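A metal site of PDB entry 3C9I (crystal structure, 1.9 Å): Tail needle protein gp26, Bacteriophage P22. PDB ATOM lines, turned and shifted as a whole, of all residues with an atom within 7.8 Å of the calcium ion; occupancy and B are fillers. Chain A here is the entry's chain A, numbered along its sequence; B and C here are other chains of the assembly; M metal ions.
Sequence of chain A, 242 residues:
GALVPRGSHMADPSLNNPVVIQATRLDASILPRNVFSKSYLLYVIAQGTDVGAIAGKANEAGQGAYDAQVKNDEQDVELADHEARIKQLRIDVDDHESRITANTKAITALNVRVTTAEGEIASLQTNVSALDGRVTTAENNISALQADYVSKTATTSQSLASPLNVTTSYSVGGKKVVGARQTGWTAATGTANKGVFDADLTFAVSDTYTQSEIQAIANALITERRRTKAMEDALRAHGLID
The backbone carbonyl oxygen (O) of Ala 68 of chain C is in hydrogen-bond range of the side-chain amide nitrogen (ND2) of Asn 72 of chain B (3.3 Å). OD1 of Asp 76 of chain C sits at hydrogen-bond distance from NE2 of Gln 75 of chain A, at 2.9 Å. O of Ala 68 of chain A is in hydrogen-bond range of ND2 of Asn 72 of chain C. The backbone carbonyl oxygen (O) of Ala 68 of chain B sits at hydrogen-bond distance from the side-chain amide nitrogen (ND2) of Asn 72 of chain A, at 3.2 Å. OD1 of Asp 76 of chain A lies within hydrogen-bond range of NE2 of Gln 75 of chain B, 2.9 Å away. NE2 of Gln 75 of chain C is in hydrogen-bond range of OD1 of Asp 76 of chain B (2.5 Å).
The nearest printed residue that does not touch the calcium ion is Lys 71 of chain C (5.3 Å).
The calcium ion is bound by the side-chain amide oxygen (OD1) of Asn 72 of chain B (2.3 Å), the side-chain amide oxygen (OE1) of Gln 75 of chain A (2.3 Å), the side-chain amide oxygen (OD1) of Asn 72 of chain C (2.3 Å), the side-chain amide oxygen (OD1) of Asn 72 of chain A (2.4 Å), the side-chain amide oxygen (OE1) of Gln 75 of chain B (2.4 Å) and the side-chain amide oxygen (OE1) of Gln 75 of chain C (2.5 Å).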
ATOM      1  N   ALA A  68      32.054 -19.400  17.087  1.00  0.00           N
ATOM      2  CA  ALA A  68      31.404 -19.949  15.907  1.00  0.00           C
ATOM      3  C   ALA A  68      32.384 -19.970  14.726  1.00  0.00           C
ATOM      4  O   ALA A  68      32.437 -20.933  13.985  1.00  0.00           O
ATOM      5  CB  ALA A  68      30.182 -19.131  15.553  1.00  0.00           C
ATOM      6  N   GLN A  69      33.129 -18.885  14.572  1.00  0.00           N
ATOM      7  CA  GLN A  69      34.100 -18.788  13.488  1.00  0.00           C
ATOM      8  C   GLN A  69      35.283 -19.726  13.690  1.00  0.00           C
ATOM      9  O   GLN A  69      35.811 -20.262  12.734  1.00  0.00           O
ATOM     10  CB  GLN A  69      34.583 -17.339  13.343  1.00  0.00           C
ATOM     11  CG  GLN A  69      33.559 -16.431  12.658  1.00  0.00           C
ATOM     12  CD  GLN A  69      34.058 -15.000  12.452  1.00  0.00           C
ATOM     13  OE1 GLN A  69      33.297 -14.129  12.028  1.00  0.00           O
ATOM     14  NE2 GLN A  69      35.333 -14.761  12.728  1.00  0.00           N
ATOM     15  N   LYS A  71      35.120 -22.555  15.204  1.00  0.00           N
ATOM     16  CA  LYS A  71      34.573 -23.869  14.923  1.00  0.00           C
ATOM     17  C   LYS A  71      34.396 -23.999  13.383  1.00  0.00           C
ATOM     18  O   LYS A  71      34.577 -25.088  12.823  1.00  0.00           O
ATOM     19  CB  LYS A  71      33.232 -24.033  15.645  1.00  0.00           C
ATOM     20  CG  LYS A  71      32.396 -25.222  15.210  1.00  0.00           C
ATOM     21  CD  LYS A  71      32.493 -26.399  16.186  1.00  0.00           C
ATOM     22  CE  LYS A  71      33.848 -27.089  16.121  1.00  0.00           C
ATOM     23  NZ  LYS A  71      33.875 -28.328  16.953  1.00  0.00           N
ATOM     24  N   ASN A  72      34.057 -22.894  12.711  1.00  0.00           N
ATOM     25  CA  ASN A  72      33.892 -22.935  11.256  1.00  0.00           C
ATOM     26  C   ASN A  72      35.228 -23.273  10.583  1.00  0.00           C
ATOM     27  O   ASN A  72      35.268 -23.992   9.586  1.00  0.00           O
ATOM     28  CB  ASN A  72      33.401 -21.603  10.691  1.00  0.00           C
ATOM     29  CG  ASN A  72      31.879 -21.512  10.658  1.00  0.00           C
ATOM     30  OD1 ASN A  72      31.211 -22.521  10.759  1.00  0.00           O
ATOM     31  ND2 ASN A  72      31.357 -20.301  10.518  1.00  0.00           N
ATOM     32  N   ASP A  73      36.318 -22.732  11.140  1.00  0.00           N
ATOM     33  CA  ASP A  73      37.637 -23.003  10.579  1.00  0.00           C
ATOM     34  C   ASP A  73      37.974 -24.477  10.714  1.00  0.00           C
ATOM     35  O   ASP A  73      38.455 -25.098   9.781  1.00  0.00           O
ATOM     36  CB  ASP A  73      38.703 -22.166  11.295  1.00  0.00           C
ATOM     37  CG  ASP A  73      38.636 -20.689  10.928  1.00  0.00           C
ATOM     38  OD1 ASP A  73      39.370 -19.891  11.535  1.00  0.00           O
ATOM     39  OD2 ASP A  73      37.846 -20.322  10.038  1.00  0.00           O
ATOM     40  N   GLN A  75      35.948 -26.862  10.925  1.00  0.00           N
ATOM     41  CA  GLN A  75      35.089 -27.642  10.049  1.00  0.00           C
ATOM     42  C   GLN A  75      35.531 -27.522   8.602  1.00  0.00           C
ATOM     43  O   GLN A  75      35.361 -28.470   7.836  1.00  0.00           O
ATOM     44  CB  GLN A  75      33.629 -27.190  10.185  1.00  0.00           C
ATOM     45  CG  GLN A  75      33.052 -27.408  11.574  1.00  0.00           C
ATOM     46  CD  GLN A  75      31.601 -27.024  11.629  1.00  0.00           C
ATOM     47  OE1 GLN A  75      31.171 -26.145  10.896  1.00  0.00           O
ATOM     48  NE2 GLN A  75      30.841 -27.654  12.505  1.00  0.00           N
ATOM     49  N   ASP A  76      36.077 -26.375   8.216  1.00  0.00           N
ATOM     50  CA  ASP A  76      36.552 -26.195   6.842  1.00  0.00           C
ATOM     51  C   ASP A  76      37.731 -27.134   6.589  1.00  0.00           C
ATOM     52  O   ASP A  76      37.891 -27.641   5.481  1.00  0.00           O
ATOM     53  CB  ASP A  76      37.005 -24.746   6.595  1.00  0.00           C
ATOM     54  CG  ASP A  76      35.857 -23.822   6.212  1.00  0.00           C
ATOM     55  OD1 ASP A  76      34.812 -24.312   5.711  1.00  0.00           O
ATOM     56  OD2 ASP A  76      35.997 -22.594   6.392  1.00  0.00           O
ATOM     57  N   LEU A  79      36.323 -30.639   6.269  1.00  0.00           N
ATOM     58  CA  LEU A  79      35.628 -30.739   4.993  1.00  0.00           C
ATOM     59  C   LEU A  79      36.663 -30.897   3.887  1.00  0.00           C
ATOM     60  O   LEU A  79      36.473 -31.703   2.975  1.00  0.00           O
ATOM     61  CB  LEU A  79      34.777 -29.497   4.751  1.00  0.00           C
ATOM     62  CG  LEU A  79      33.403 -29.422   5.467  1.00  0.00           C
ATOM     63  CD1 LEU A  79      32.733 -28.088   5.215  1.00  0.00           C
ATOM     64  CD2 LEU A  79      32.516 -30.554   4.978  1.00  0.00           C
ATOM     65  N   MET B  10      20.283 -19.438   6.002  1.00  0.00           N
ATOM     66  CA  MET B  10      19.854 -18.892   7.285  1.00  0.00           C
ATOM     67  C   MET B  10      20.435 -17.505   7.545  1.00  0.00           C
ATOM     68  O   MET B  10      19.901 -16.745   8.345  1.00  0.00           O
ATOM     69  CB  MET B  10      20.269 -19.830   8.434  1.00  0.00           C
ATOM     70  CG  MET B  10      21.777 -19.867   8.759  1.00  0.00           C
ATOM     71  SD  MET B  10      22.101 -20.403  10.494  1.00  0.00           S
ATOM     72  CE  MET B  10      23.836 -20.579  10.517  1.00  0.00           C
ATOM     73  N   ALA B  68      29.736 -15.870  10.137  1.00  0.00           N
ATOM     74  CA  ALA B  68      29.721 -17.272  10.514  1.00  0.00           C
ATOM     75  C   ALA B  68      28.507 -17.970   9.867  1.00  0.00           C
ATOM     76  O   ALA B  68      28.606 -19.118   9.441  1.00  0.00           O
ATOM     77  CB  ALA B  68      29.677 -17.417  12.049  1.00  0.00           C
ATOM     78  N   GLN B  69      27.383 -17.252   9.796  1.00  0.00           N
ATOM     79  CA  GLN B  69      26.166 -17.801   9.216  1.00  0.00           C
ATOM     80  C   GLN B  69      26.287 -17.982   7.698  1.00  0.00           C
ATOM     81  O   GLN B  69      25.852 -18.992   7.163  1.00  0.00           O
ATOM     82  CB  GLN B  69      24.961 -16.926   9.568  1.00  0.00           C
ATOM     83  CG  GLN B  69      24.616 -16.930  11.060  1.00  0.00           C
ATOM     84  CD  GLN B  69      23.274 -16.285  11.404  1.00  0.00           C
ATOM     85  OE1 GLN B  69      22.891 -16.214  12.580  1.00  0.00           O
ATOM     86  NE2 GLN B  69      22.544 -15.811  10.393  1.00  0.00           N
ATOM     87  N   LYS B  71      28.936 -18.525   6.118  1.00  0.00           N
ATOM     88  CA  LYS B  71      29.839 -19.666   5.996  1.00  0.00           C
ATOM     89  C   LYS B  71      29.085 -20.965   6.309  1.00  0.00           C
ATOM     90  O   LYS B  71      29.314 -21.989   5.652  1.00  0.00           O
ATOM     91  CB  LYS B  71      31.018 -19.467   6.958  1.00  0.00           C
ATOM     92  CG  LYS B  71      31.871 -20.708   7.142  1.00  0.00           C
ATOM     93  CD  LYS B  71      32.665 -21.040   5.906  1.00  0.00           C
ATOM     94  CE  LYS B  71      33.866 -20.116   5.761  1.00  0.00           C
ATOM     95  NZ  LYS B  71      34.706 -20.537   4.608  1.00  0.00           N
ATOM     96  N   ASN B  72      28.197 -20.945   7.310  1.00  0.00           N
ATOM     97  CA  ASN B  72      27.437 -22.155   7.625  1.00  0.00           C
ATOM     98  C   ASN B  72      26.633 -22.564   6.414  1.00  0.00           C
ATOM     99  O   ASN B  72      26.571 -23.744   6.109  1.00  0.00           O
ATOM    100  CB  ASN B  72      26.482 -21.932   8.788  1.00  0.00           C
ATOM    101  CG  ASN B  72      27.143 -22.146  10.105  1.00  0.00           C
ATOM    102  OD1 ASN B  72      28.243 -22.655  10.161  1.00  0.00           O
ATOM    103  ND2 ASN B  72      26.470 -21.742  11.186  1.00  0.00           N
ATOM    104  N   ASP B  73      26.000 -21.599   5.747  1.00  0.00           N
ATOM    105  CA  ASP B  73      25.218 -21.917   4.568  1.00  0.00           C
ATOM    106  C   ASP B  73      26.084 -22.579   3.487  1.00  0.00           C
ATOM    107  O   ASP B  73      25.657 -23.557   2.864  1.00  0.00           O
ATOM    108  CB  ASP B  73      24.557 -20.657   4.032  1.00  0.00           C
ATOM    109  CG  ASP B  73      23.385 -20.201   4.902  1.00  0.00           C
ATOM    110  OD1 ASP B  73      22.863 -19.079   4.697  1.00  0.00           O
ATOM    111  OD2 ASP B  73      22.971 -20.979   5.789  1.00  0.00           O
ATOM    112  N   GLN B  75      28.835 -24.301   3.982  1.00  0.00           N
ATOM    113  CA  GLN B  75      29.252 -25.617   4.441  1.00  0.00           C
ATOM    114  C   GLN B  75      28.113 -26.612   4.347  1.00  0.00           C
ATOM    115  O   GLN B  75      28.346 -27.807   4.195  1.00  0.00           O
ATOM    116  CB  GLN B  75      29.768 -25.542   5.886  1.00  0.00           C
ATOM    117  CG  GLN B  75      31.070 -24.777   6.022  1.00  0.00           C
ATOM    118  CD  GLN B  75      31.450 -24.592   7.482  1.00  0.00           C
ATOM    119  OE1 GLN B  75      30.585 -24.527   8.335  1.00  0.00           O
ATOM    120  NE2 GLN B  75      32.742 -24.482   7.761  1.00  0.00           N
ATOM    121  N   ASP B  76      26.872 -26.115   4.437  1.00  0.00           N
ATOM    122  CA  ASP B  76      25.725 -26.991   4.310  1.00  0.00           C
ATOM    123  C   ASP B  76      25.685 -27.534   2.868  1.00  0.00           C
ATOM    124  O   ASP B  76      25.420 -28.721   2.657  1.00  0.00           O
ATOM    125  CB  ASP B  76      24.433 -26.221   4.622  1.00  0.00           C
ATOM    126  CG  ASP B  76      24.011 -26.379   6.079  1.00  0.00           C
ATOM    127  OD1 ASP B  76      24.778 -26.976   6.858  1.00  0.00           O
ATOM    128  OD2 ASP B  76      22.904 -25.919   6.444  1.00  0.00           O
ATOM    129  N   LEU B  79      28.324 -30.181   2.636  1.00  0.00           N
ATOM    130  CA  LEU B  79      27.947 -31.375   3.390  1.00  0.00           C
ATOM    131  C   LEU B  79      26.958 -32.256   2.613  1.00  0.00           C
ATOM    132  O   LEU B  79      27.092 -33.480   2.598  1.00  0.00           O
ATOM    133  CB  LEU B  79      27.343 -30.992   4.752  1.00  0.00           C
ATOM    134  CG  LEU B  79      28.361 -30.728   5.865  1.00  0.00           C
ATOM    135  CD1 LEU B  79      27.675 -30.096   7.059  1.00  0.00           C
ATOM    136  CD2 LEU B  79      29.058 -32.003   6.256  1.00  0.00           C
ATOM    137  N   ALA C  68      24.200 -19.542  14.807  1.00  0.00           N
ATOM    138  CA  ALA C  68      25.390 -20.091  14.157  1.00  0.00           C
ATOM    139  C   ALA C  68      25.922 -21.276  14.960  1.00  0.00           C
ATOM    140  O   ALA C  68      26.259 -22.324  14.396  1.00  0.00           O
ATOM    141  CB  ALA C  68      26.470 -19.015  14.039  1.00  0.00           C
ATOM    142  N   GLN C  69      25.977 -21.119  16.280  1.00  0.00           N
ATOM    143  CA  GLN C  69      26.473 -22.206  17.114  1.00  0.00           C
ATOM    144  C   GLN C  69      25.567 -23.447  17.011  1.00  0.00           C
ATOM    145  O   GLN C  69      26.049 -24.575  16.857  1.00  0.00           O
ATOM    146  CB  GLN C  69      26.601 -21.747  18.572  1.00  0.00           C
ATOM    147  CG  GLN C  69      27.644 -20.629  18.767  1.00  0.00           C
ATOM    148  CD  GLN C  69      28.029 -20.374  20.234  1.00  0.00           C
ATOM    149  OE1 GLN C  69      27.376 -20.857  21.152  1.00  0.00           O
ATOM    150  NE2 GLN C  69      29.099 -19.615  20.435  1.00  0.00           N
ATOM    151  N   LYS C  71      23.778 -24.317  14.577  1.00  0.00           N
ATOM    152  CA  LYS C  71      24.007 -24.936  13.280  1.00  0.00           C
ATOM    153  C   LYS C  71      25.347 -25.690  13.297  1.00  0.00           C
ATOM    154  O   LYS C  71      25.472 -26.772  12.713  1.00  0.00           O
ATOM    155  CB  LYS C  71      23.956 -23.854  12.184  1.00  0.00           C
ATOM    156  CG  LYS C  71      24.466 -24.293  10.805  1.00  0.00           C
ATOM    157  CD  LYS C  71      23.656 -25.406  10.177  1.00  0.00           C
ATOM    158  CE  LYS C  71      22.254 -24.939   9.780  1.00  0.00           C
ATOM    159  NZ  LYS C  71      21.584 -25.958   8.927  1.00  0.00           N
ATOM    160  N   ASN C  72      26.354 -25.136  13.981  1.00  0.00           N
ATOM    161  CA  ASN C  72      27.648 -25.813  14.044  1.00  0.00           C
ATOM    162  C   ASN C  72      27.541 -27.197  14.673  1.00  0.00           C
ATOM    163  O   ASN C  72      28.142 -28.149  14.190  1.00  0.00           O
ATOM    164  CB  ASN C  72      28.665 -25.011  14.858  1.00  0.00           C
ATOM    165  CG  ASN C  72      29.331 -23.948  14.056  1.00  0.00           C
ATOM    166  OD1 ASN C  72      29.336 -24.032  12.839  1.00  0.00           O
ATOM    167  ND2 ASN C  72      29.905 -22.941  14.727  1.00  0.00           N
ATOM    168  N   ASP C  73      26.773 -27.290  15.757  1.00  0.00           N
ATOM    169  CA  ASP C  73      26.572 -28.551  16.465  1.00  0.00           C
ATOM    170  C   ASP C  73      25.987 -29.604  15.557  1.00  0.00           C
ATOM    171  O   ASP C  73      26.383 -30.771  15.594  1.00  0.00           O
ATOM    172  CB  ASP C  73      25.631 -28.358  17.645  1.00  0.00           C
ATOM    173  CG  ASP C  73      26.238 -27.519  18.757  1.00  0.00           C
ATOM    174  OD1 ASP C  73      25.557 -27.345  19.795  1.00  0.00           O
ATOM    175  OD2 ASP C  73      27.371 -27.029  18.588  1.00  0.00           O
ATOM    176  N   GLN C  75      26.158 -29.613  12.236  1.00  0.00           N
ATOM    177  CA  GLN C  75      27.118 -29.969  11.187  1.00  0.00           C
ATOM    178  C   GLN C  75      28.228 -30.829  11.752  1.00  0.00           C
ATOM    179  O   GLN C  75      28.876 -31.573  11.015  1.00  0.00           O
ATOM    180  CB  GLN C  75      27.698 -28.714  10.521  1.00  0.00           C
ATOM    181  CG  GLN C  75      26.683 -27.922   9.703  1.00  0.00           C
ATOM    182  CD  GLN C  75      27.193 -26.566   9.284  1.00  0.00           C
ATOM    183  OE1 GLN C  75      27.900 -25.924  10.054  1.00  0.00           O
ATOM    184  NE2 GLN C  75      26.832 -26.114   8.092  1.00  0.00           N
ATOM    185  N   ASP C  76      28.474 -30.730  13.060  1.00  0.00           N
ATOM    186  CA  ASP C  76      29.500 -31.567  13.680  1.00  0.00           C
ATOM    187  C   ASP C  76      28.981 -32.995  13.695  1.00  0.00           C
ATOM    188  O   ASP C  76      29.690 -33.935  13.413  1.00  0.00           O
ATOM    189  CB  ASP C  76      29.826 -31.104  15.110  1.00  0.00           C
ATOM    190  CG  ASP C  76      31.017 -30.154  15.163  1.00  0.00           C
ATOM    191  OD1 ASP C  76      31.659 -29.919  14.115  1.00  0.00           O
ATOM    192  OD2 ASP C  76      31.326 -29.635  16.265  1.00  0.00           O
ATOM    193  N   LEU C  79      29.420 -34.266  10.193  1.00  0.00           N
ATOM    194  CA  LEU C  79      30.824 -34.507   9.867  1.00  0.00           C
ATOM    195  C   LEU C  79      31.342 -35.818  10.463  1.00  0.00           C
ATOM    196  O   LEU C  79      32.112 -36.536   9.829  1.00  0.00           O
ATOM    197  CB  LEU C  79      31.683 -33.327  10.340  1.00  0.00           C
ATOM    198  CG  LEU C  79      31.649 -32.088   9.444  1.00  0.00           C
ATOM    199  CD1 LEU C  79      32.101 -30.821  10.209  1.00  0.00           C
ATOM    200  CD2 LEU C  79      32.547 -32.344   8.244  1.00  0.00           C
HETATM  201 CA    CA M   1      29.746 -24.358  10.556  1.00  0.00          CA
